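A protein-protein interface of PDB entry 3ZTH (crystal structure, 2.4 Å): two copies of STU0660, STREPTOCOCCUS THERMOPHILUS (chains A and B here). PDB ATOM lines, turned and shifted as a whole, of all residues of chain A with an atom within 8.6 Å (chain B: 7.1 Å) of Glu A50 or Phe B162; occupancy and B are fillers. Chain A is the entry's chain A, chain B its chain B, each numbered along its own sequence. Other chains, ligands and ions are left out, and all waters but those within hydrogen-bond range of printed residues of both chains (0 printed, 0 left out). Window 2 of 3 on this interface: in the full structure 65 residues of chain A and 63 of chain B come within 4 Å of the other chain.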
ATOM      1  N   TRP A  40       3.942  17.031  24.450  1.00  0.00           N
ATOM      2  CA  TRP A  40       2.702  17.800  24.473  1.00  0.00           C
ATOM      3  C   TRP A  40       2.873  19.040  25.329  1.00  0.00           C
ATOM      4  O   TRP A  40       2.503  20.137  24.931  1.00  0.00           O
ATOM      5  CB  TRP A  40       1.559  16.950  25.024  1.00  0.00           C
ATOM      6  CG  TRP A  40       0.871  16.109  23.987  1.00  0.00           C
ATOM      7  CD1 TRP A  40       1.304  15.846  22.713  1.00  0.00           C
ATOM      8  CD2 TRP A  40      -0.379  15.418  24.135  1.00  0.00           C
ATOM      9  NE1 TRP A  40       0.401  15.036  22.063  1.00  0.00           N
ATOM     10  CE2 TRP A  40      -0.641  14.759  22.909  1.00  0.00           C
ATOM     11  CE3 TRP A  40      -1.303  15.293  25.184  1.00  0.00           C
ATOM     12  CZ2 TRP A  40      -1.794  13.986  22.705  1.00  0.00           C
ATOM     13  CZ3 TRP A  40      -2.449  14.524  24.980  1.00  0.00           C
ATOM     14  CH2 TRP A  40      -2.682  13.882  23.747  1.00  0.00           C
ATOM     15  N   LYS A  45       1.001  21.680  22.557  1.00  0.00           N
ATOM     16  CA  LYS A  45      -0.229  20.956  22.287  1.00  0.00           C
ATOM     17  C   LYS A  45      -1.468  21.696  22.800  1.00  0.00           C
ATOM     18  O   LYS A  45      -1.500  22.169  23.934  1.00  0.00           O
ATOM     19  CB  LYS A  45      -0.156  19.577  22.944  1.00  0.00           C
ATOM     20  CG  LYS A  45      -1.427  18.767  22.877  1.00  0.00           C
ATOM     21  CD  LYS A  45      -1.671  18.234  21.484  1.00  0.00           C
ATOM     22  CE  LYS A  45      -2.838  17.250  21.479  1.00  0.00           C
ATOM     23  NZ  LYS A  45      -2.997  16.575  20.158  1.00  0.00           N
ATOM     24  N   TYR A  47      -4.933  21.105  23.975  1.00  0.00           N
ATOM     25  CA  TYR A  47      -5.701  19.985  24.486  1.00  0.00           C
ATOM     26  C   TYR A  47      -7.193  19.963  24.204  1.00  0.00           C
ATOM     27  O   TYR A  47      -7.892  20.952  24.418  1.00  0.00           O
ATOM     28  CB  TYR A  47      -5.518  19.893  25.995  1.00  0.00           C
ATOM     29  CG  TYR A  47      -4.086  19.955  26.474  1.00  0.00           C
ATOM     30  CD1 TYR A  47      -3.163  18.971  26.116  1.00  0.00           C
ATOM     31  CD2 TYR A  47      -3.673  20.962  27.345  1.00  0.00           C
ATOM     32  CE1 TYR A  47      -1.858  18.983  26.623  1.00  0.00           C
ATOM     33  CE2 TYR A  47      -2.379  20.986  27.854  1.00  0.00           C
ATOM     34  CZ  TYR A  47      -1.477  19.992  27.494  1.00  0.00           C
ATOM     35  OH  TYR A  47      -0.204  20.008  28.017  1.00  0.00           O
ATOM     36  N   SER A  48      -7.679  18.819  23.737  1.00  0.00           N
ATOM     37  CA  SER A  48      -9.103  18.647  23.496  1.00  0.00           C
ATOM     38  C   SER A  48      -9.570  18.073  24.822  1.00  0.00           C
ATOM     39  O   SER A  48      -8.744  17.781  25.687  1.00  0.00           O
ATOM     40  CB  SER A  48      -9.358  17.630  22.388  1.00  0.00           C
ATOM     41  OG  SER A  48      -9.038  16.319  22.820  1.00  0.00           O
ATOM     42  N   SER A  49     -10.874  17.904  25.002  1.00  0.00           N
ATOM     43  CA  SER A  49     -11.361  17.347  26.256  1.00  0.00           C
ATOM     44  C   SER A  49     -11.067  15.848  26.323  1.00  0.00           C
ATOM     45  O   SER A  49     -10.907  15.288  27.404  1.00  0.00           O
ATOM     46  CB  SER A  49     -12.862  17.612  26.416  1.00  0.00           C
ATOM     47  OG  SER A  49     -13.582  17.178  25.279  1.00  0.00           O
ATOM     48  N   GLU A  50     -10.989  15.196  25.169  1.00  0.00           N
ATOM     49  CA  GLU A  50     -10.687  13.770  25.150  1.00  0.00           C
ATOM     50  C   GLU A  50      -9.222  13.556  25.538  1.00  0.00           C
ATOM     51  O   GLU A  50      -8.844  12.482  26.007  1.00  0.00           O
ATOM     52  CB  GLU A  50     -10.955  13.165  23.764  1.00  0.00           C
ATOM     53  CG  GLU A  50     -12.434  13.030  23.396  1.00  0.00           C
ATOM     54  CD  GLU A  50     -13.013  14.284  22.746  1.00  0.00           C
ATOM     55  OE1 GLU A  50     -12.872  15.385  23.318  1.00  0.00           O
ATOM     56  OE2 GLU A  50     -13.619  14.164  21.660  1.00  0.00           O
ATOM     57  N   ASP A  51      -8.400  14.583  25.341  1.00  0.00           N
ATOM     58  CA  ASP A  51      -6.993  14.485  25.694  1.00  0.00           C
ATOM     59  C   ASP A  51      -6.839  14.560  27.205  1.00  0.00           C
ATOM     60  O   ASP A  51      -5.998  13.880  27.787  1.00  0.00           O
ATOM     61  CB  ASP A  51      -6.184  15.629  25.073  1.00  0.00           C
ATOM     62  CG  ASP A  51      -6.121  15.565  23.560  1.00  0.00           C
ATOM     63  OD1 ASP A  51      -6.058  14.457  23.000  1.00  0.00           O
ATOM     64  OD2 ASP A  51      -6.109  16.638  22.930  1.00  0.00           O
ATOM     65  N   LEU A  52      -7.661  15.387  27.842  1.00  0.00           N
ATOM     66  CA  LEU A  52      -7.586  15.573  29.290  1.00  0.00           C
ATOM     67  C   LEU A  52      -8.427  14.595  30.110  1.00  0.00           C
ATOM     68  O   LEU A  52      -8.415  14.644  31.341  1.00  0.00           O
ATOM     69  CB  LEU A  52      -7.967  17.013  29.631  1.00  0.00           C
ATOM     70  CG  LEU A  52      -7.127  18.049  28.874  1.00  0.00           C
ATOM     71  CD1 LEU A  52      -7.694  19.439  29.072  1.00  0.00           C
ATOM     72  CD2 LEU A  52      -5.687  17.986  29.358  1.00  0.00           C
ATOM     73  N   SER A  53      -9.140  13.701  29.427  1.00  0.00           N
ATOM     74  CA  SER A  53      -9.988  12.704  30.085  1.00  0.00           C
ATOM     75  C   SER A  53      -9.312  12.080  31.296  1.00  0.00           C
ATOM     76  O   SER A  53      -9.786  12.218  32.417  1.00  0.00           O
ATOM     77  CB  SER A  53     -10.342  11.584  29.112  1.00  0.00           C
ATOM     78  OG  SER A  53     -10.872  12.117  27.918  1.00  0.00           O
ATOM     79  N   ILE A  54      -8.201  11.392  31.048  1.00  0.00           N
ATOM     80  CA  ILE A  54      -7.436  10.710  32.088  1.00  0.00           C
ATOM     81  C   ILE A  54      -6.924  11.608  33.216  1.00  0.00           C
ATOM     82  O   ILE A  54      -6.494  11.118  34.260  1.00  0.00           O
ATOM     83  CB  ILE A  54      -6.223   9.968  31.478  1.00  0.00           C
ATOM     84  CG1 ILE A  54      -5.275  10.975  30.819  1.00  0.00           C
ATOM     85  CG2 ILE A  54      -6.703   8.932  30.485  1.00  0.00           C
ATOM     86  CD1 ILE A  54      -3.969  10.378  30.317  1.00  0.00           C
ATOM     87  N   PHE A  55      -6.947  12.916  33.015  1.00  0.00           N
ATOM     88  CA  PHE A  55      -6.482  13.807  34.060  1.00  0.00           C
ATOM     89  C   PHE A  55      -7.672  14.543  34.666  1.00  0.00           C
ATOM     90  O   PHE A  55      -7.520  15.605  35.265  1.00  0.00           O
ATOM     91  CB  PHE A  55      -5.488  14.809  33.481  1.00  0.00           C
ATOM     92  CG  PHE A  55      -4.296  14.173  32.838  1.00  0.00           C
ATOM     93  CD1 PHE A  55      -3.383  13.449  33.597  1.00  0.00           C
ATOM     94  CD2 PHE A  55      -4.088  14.287  31.465  1.00  0.00           C
ATOM     95  CE1 PHE A  55      -2.278  12.848  32.999  1.00  0.00           C
ATOM     96  CE2 PHE A  55      -2.986  13.688  30.859  1.00  0.00           C
ATOM     97  CZ  PHE A  55      -2.081  12.969  31.627  1.00  0.00           C
ATOM     98  N   TYR A  57     -10.109  16.026  33.063  1.00  0.00           N
ATOM     99  CA  TYR A  57     -10.316  17.240  32.277  1.00  0.00           C
ATOM    100  C   TYR A  57      -9.534  18.443  32.781  1.00  0.00           C
ATOM    101  O   TYR A  57      -9.921  19.590  32.553  1.00  0.00           O
ATOM    102  CB  TYR A  57     -11.809  17.543  32.224  1.00  0.00           C
ATOM    103  CG  TYR A  57     -12.581  16.348  31.724  1.00  0.00           C
ATOM    104  CD1 TYR A  57     -12.624  16.044  30.363  1.00  0.00           C
ATOM    105  CD2 TYR A  57     -13.181  15.456  32.619  1.00  0.00           C
ATOM    106  CE1 TYR A  57     -13.236  14.882  29.902  1.00  0.00           C
ATOM    107  CE2 TYR A  57     -13.792  14.292  32.171  1.00  0.00           C
ATOM    108  CZ  TYR A  57     -13.815  14.011  30.811  1.00  0.00           C
ATOM    109  OH  TYR A  57     -14.400  12.856  30.359  1.00  0.00           O
ATOM    110  N   TYR B  92     -12.104   7.259   9.286  1.00  0.00           N
ATOM    111  CA  TYR B  92     -12.911   7.069   8.092  1.00  0.00           C
ATOM    112  C   TYR B  92     -12.623   8.118   7.032  1.00  0.00           C
ATOM    113  O   TYR B  92     -13.295   9.139   6.951  1.00  0.00           O
ATOM    114  CB  TYR B  92     -14.386   7.066   8.478  1.00  0.00           C
ATOM    115  CG  TYR B  92     -14.722   5.895   9.367  1.00  0.00           C
ATOM    116  CD1 TYR B  92     -15.070   4.661   8.822  1.00  0.00           C
ATOM    117  CD2 TYR B  92     -14.608   5.992  10.752  1.00  0.00           C
ATOM    118  CE1 TYR B  92     -15.290   3.550   9.631  1.00  0.00           C
ATOM    119  CE2 TYR B  92     -14.825   4.886  11.572  1.00  0.00           C
ATOM    120  CZ  TYR B  92     -15.164   3.667  11.006  1.00  0.00           C
ATOM    121  OH  TYR B  92     -15.361   2.562  11.809  1.00  0.00           O
ATOM    122  N   PHE B 159     -22.526  11.522  12.821  1.00  0.00           N
ATOM    123  CA  PHE B 159     -21.719  10.417  13.318  1.00  0.00           C
ATOM    124  C   PHE B 159     -20.252  10.777  13.425  1.00  0.00           C
ATOM    125  O   PHE B 159     -19.679  11.372  12.510  1.00  0.00           O
ATOM    126  CB  PHE B 159     -21.860   9.202  12.408  1.00  0.00           C
ATOM    127  CG  PHE B 159     -23.117   8.437  12.625  1.00  0.00           C
ATOM    128  CD1 PHE B 159     -23.340   7.780  13.829  1.00  0.00           C
ATOM    129  CD2 PHE B 159     -24.090   8.376  11.634  1.00  0.00           C
ATOM    130  CE1 PHE B 159     -24.520   7.072  14.039  1.00  0.00           C
ATOM    131  CE2 PHE B 159     -25.271   7.672  11.837  1.00  0.00           C
ATOM    132  CZ  PHE B 159     -25.486   7.019  13.041  1.00  0.00           C
ATOM    133  N   SER B 160     -19.657  10.403  14.552  1.00  0.00           N
ATOM    134  CA  SER B 160     -18.247  10.644  14.822  1.00  0.00           C
ATOM    135  C   SER B 160     -17.718   9.441  15.583  1.00  0.00           C
ATOM    136  O   SER B 160     -18.351   8.969  16.531  1.00  0.00           O
ATOM    137  CB  SER B 160     -18.056  11.892  15.689  1.00  0.00           C
ATOM    138  OG  SER B 160     -18.609  13.038  15.075  1.00  0.00           O
ATOM    139  N   PRO B 161     -16.553   8.922  15.172  1.00  0.00           N
ATOM    140  CA  PRO B 161     -15.932   7.767  15.827  1.00  0.00           C
ATOM    141  C   PRO B 161     -15.329   8.198  17.159  1.00  0.00           C
ATOM    142  O   PRO B 161     -14.933   9.352  17.311  1.00  0.00           O
ATOM    143  CB  PRO B 161     -14.880   7.330  14.814  1.00  0.00           C
ATOM    144  CG  PRO B 161     -14.474   8.625  14.192  1.00  0.00           C
ATOM    145  CD  PRO B 161     -15.804   9.301  13.963  1.00  0.00           C
ATOM    146  N   PHE B 162     -15.268   7.282  18.117  1.00  0.00           N
ATOM    147  CA  PHE B 162     -14.729   7.583  19.441  1.00  0.00           C
ATOM    148  C   PHE B 162     -14.080   6.387  20.115  1.00  0.00           C
ATOM    149  O   PHE B 162     -14.513   5.250  19.940  1.00  0.00           O
ATOM    150  CB  PHE B 162     -15.836   8.072  20.379  1.00  0.00           C
ATOM    151  CG  PHE B 162     -16.165   9.524  20.240  1.00  0.00           C
ATOM    152  CD1 PHE B 162     -15.269  10.495  20.673  1.00  0.00           C
ATOM    153  CD2 PHE B 162     -17.380   9.924  19.687  1.00  0.00           C
ATOM    154  CE1 PHE B 162     -15.575  11.850  20.560  1.00  0.00           C
ATOM    155  CE2 PHE B 162     -17.700  11.274  19.569  1.00  0.00           C
ATOM    156  CZ  PHE B 162     -16.793  12.241  20.008  1.00  0.00           C
ATOM    157  N   PHE B 163     -13.045   6.663  20.898  1.00  0.00           N
ATOM    158  CA  PHE B 163     -12.360   5.626  21.658  1.00  0.00           C
ATOM    159  C   PHE B 163     -12.885   5.819  23.073  1.00  0.00           C
ATOM    160  O   PHE B 163     -12.869   6.932  23.602  1.00  0.00           O
ATOM    161  CB  PHE B 163     -10.842   5.826  21.609  1.00  0.00           C
ATOM    162  CG  PHE B 163     -10.221   5.375  20.324  1.00  0.00           C
ATOM    163  CD1 PHE B 163     -10.035   4.017  20.067  1.00  0.00           C
ATOM    164  CD2 PHE B 163      -9.877   6.296  19.343  1.00  0.00           C
ATOM    165  CE1 PHE B 163      -9.514   3.579  18.843  1.00  0.00           C
ATOM    166  CE2 PHE B 163      -9.358   5.873  18.116  1.00  0.00           C
ATOM    167  CZ  PHE B 163      -9.176   4.511  17.865  1.00  0.00           C
ATOM    168  N   ALA B 164     -13.371   4.748  23.683  1.00  0.00           N
ATOM    169  CA  ALA B 164     -13.912   4.890  25.018  1.00  0.00           C
ATOM    170  C   ALA B 164     -13.816   3.660  25.894  1.00  0.00           C
ATOM    171  O   ALA B 164     -13.732   2.523  25.419  1.00  0.00           O
ATOM    172  CB  ALA B 164     -15.373   5.346  24.933  1.00  0.00           C
ATOM    173  N   ASN B 169     -15.162   8.642  26.561  1.00  0.00           N
ATOM    174  CA  ASN B 169     -14.192   8.853  25.500  1.00  0.00           C
ATOM    175  C   ASN B 169     -12.841   9.376  25.973  1.00  0.00           C
ATOM    176  O   ASN B 169     -12.748  10.145  26.933  1.00  0.00           O
ATOM    177  CB  ASN B 169     -14.749   9.822  24.452  1.00  0.00           C
ATOM    178  CG  ASN B 169     -16.140   9.443  23.983  1.00  0.00           C
ATOM    179  OD1 ASN B 169     -16.534   8.274  24.039  1.00  0.00           O
ATOM    180  ND2 ASN B 169     -16.888  10.430  23.504  1.00  0.00           N
ATOM    181  N   LEU B 170     -11.796   8.931  25.286  1.00  0.00           N
ATOM    182  CA  LEU B 170     -10.434   9.369  25.548  1.00  0.00           C
ATOM    183  C   LEU B 170      -9.714   9.386  24.209  1.00  0.00           C
ATOM    184  O   LEU B 170     -10.128   8.707  23.267  1.00  0.00           O
ATOM    185  CB  LEU B 170      -9.705   8.443  26.534  1.00  0.00           C
ATOM    186  CG  LEU B 170      -9.707   6.916  26.453  1.00  0.00           C
ATOM    187  CD1 LEU B 170      -9.671   6.426  25.021  1.00  0.00           C
ATOM    188  CD2 LEU B 170      -8.496   6.406  27.242  1.00  0.00           C
ATOM    189  N   SER B 171      -8.651  10.173  24.124  1.00  0.00           N
ATOM    190  CA  SER B 171      -7.886  10.277  22.894  1.00  0.00           C
ATOM    191  C   SER B 171      -7.087   9.008  22.606  1.00  0.00           C
ATOM    192  O   SER B 171      -6.584   8.348  23.517  1.00  0.00           O
ATOM    193  CB  SER B 171      -6.955  11.484  22.973  1.00  0.00           C
ATOM    194  OG  SER B 171      -7.706  12.668  23.171  1.00  0.00           O
ATOM    195  N   PHE B 172      -6.989   8.670  21.324  1.00  0.00           N
ATOM    196  CA  PHE B 172      -6.261   7.487  20.878  1.00  0.00           C
ATOM    197  C   PHE B 172      -4.904   7.347  21.562  1.00  0.00           C
ATOM    198  O   PHE B 172      -4.452   6.237  21.846  1.00  0.00           O
ATOM    199  CB  PHE B 172      -6.053   7.547  19.363  1.00  0.00           C
ATOM    200  CG  PHE B 172      -5.188   6.445  18.826  1.00  0.00           C
ATOM    201  CD1 PHE B 172      -5.666   5.143  18.748  1.00  0.00           C
ATOM    202  CD2 PHE B 172      -3.887   6.712  18.403  1.00  0.00           C
ATOM    203  CE1 PHE B 172      -4.866   4.119  18.257  1.00  0.00           C
ATOM    204  CE2 PHE B 172      -3.078   5.695  17.911  1.00  0.00           C
ATOM    205  CZ  PHE B 172      -3.568   4.392  17.836  1.00  0.00           C
ATOM    206  N   TRP B 174      -4.053   7.873  24.554  1.00  0.00           N
ATOM    207  CA  TRP B 174      -4.126   7.289  25.896  1.00  0.00           C
ATOM    208  C   TRP B 174      -4.577   5.828  25.965  1.00  0.00           C
ATOM    209  O   TRP B 174      -4.623   5.230  27.046  1.00  0.00           O
ATOM    210  CB  TRP B 174      -5.011   8.171  26.780  1.00  0.00           C
ATOM    211  CG  TRP B 174      -4.478   9.580  26.895  1.00  0.00           C
ATOM    212  CD1 TRP B 174      -5.209  10.731  26.921  1.00  0.00           C
ATOM    213  CD2 TRP B 174      -3.100   9.977  27.014  1.00  0.00           C
ATOM    214  NE1 TRP B 174      -4.376  11.821  27.047  1.00  0.00           N
ATOM    215  CE2 TRP B 174      -3.079  11.389  27.108  1.00  0.00           C
ATOM    216  CE3 TRP B 174      -1.884   9.276  27.054  1.00  0.00           C
ATOM    217  CZ2 TRP B 174      -1.891  12.116  27.239  1.00  0.00           C
ATOM    218  CZ3 TRP B 174      -0.701  10.000  27.186  1.00  0.00           C
ATOM    219  CH2 TRP B 174      -0.717  11.410  27.277  1.00  0.00           C
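Of the 12 printed residues of chain B, 5 touch a printed residue of chain A.
Printed residues of chain B that touch a printed residue of chain A: Phe B162, Asn B169, Leu B170, Ser B171 and Trp B174.
Hydrophobic or aromatic side chains of chain B that line the printed part of chain A: Phe B162 and Trp B174.
Printed residues of chain A that touch a printed residue of chain B: Trp A40, Ser A48, Glu A50, Asp A51, Ser A53 and Ile A54.
Hydrophobic or aromatic side chains of chain A within 4 Å of the printed part of chain B: Trp A40 and Ile A54.
Among the printed residues, 10 pairs touch across the chains.
The side-chain hydroxyl (OG) of Ser A53 is in hydrogen-bond range of the backbone carbonyl oxygen (O) of Asn B169.
The backbone carbonyl oxygen (O) of Asp A51 is in hydrogen-bond range of the indole nitrogen (NE1) of Trp B174, 2.7 Å away.
The backbone NH (N) of Ser B171 sits at hydrogen-bond distance from the backbone carbonyl oxygen (O) of Glu A50 (3.0 Å).
OG of Ser B171 is in hydrogen-bond range of OD1 of Asp A51.
Printed residues of chain B within 4 Å of Glu A50: Phe B162 (3.2 Å), Leu B170 (3.5 Å) and Ser B171 (2.9 Å).
Printed residues of chain B within 4 Å of Asp A51: Ser B171 and Trp B174.
Printed residues of chain B within 4 Å of Ile A54: Trp B174.
Phe B162 touches just one residue of chain A: Glu A50.
Of the printed residues of chain A, Asn B169 touches Ser A53.
Printed residues of chain A within 4 Å of Leu B170: Glu A50 and Ser A53.
Of the printed residues of chain A, Ser B171 touches Ser A48, Glu A50 and Asp A51.
The nearest residue of chain B that does not touch Glu A50 is Asn B169 (4.1 Å).
The nearest residue of chain A that does not touch Phe B162 is Ser A49 (7.4 Å).
Trp A40 touches Trp B174.
Ser B171 touches Ser A48 (OG to OG, 3.9 Å).
OE2 of Glu A50 touches CE1 of Phe B162, at 3.2 Å.
O of Glu A50 touches CA of Leu B170, 3.5 Å away.
Leu B170 touches Ser A53.
CD2 of Trp B174 touches CD1 of Ile A54, 3.4 Å away.
The backbone NH of Leu B170 is in hydrogen-bond range of the backbone carbonyl oxygen of Phe B163, 2.8 Å away.
The backbone carbonyl oxygen of Ser A49 lies within hydrogen-bond range of the side-chain hydroxyl of Ser A53, at 3.2 Å.
OD2 of Asp A51 is in hydrogen-bond range of N of Ser A48, at 2.8 Å.
The backbone carbonyl oxygen of Glu A50 is in hydrogen-bond range of the side-chain hydroxyl of Ser A53.
O of Trp A40 sits at hydrogen-bond distance from N of Lys A45, 3.2 Å away.
OG of Ser A48 sits close to N of Glu A50 (3.3 Å).
No position is printed for both chains.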
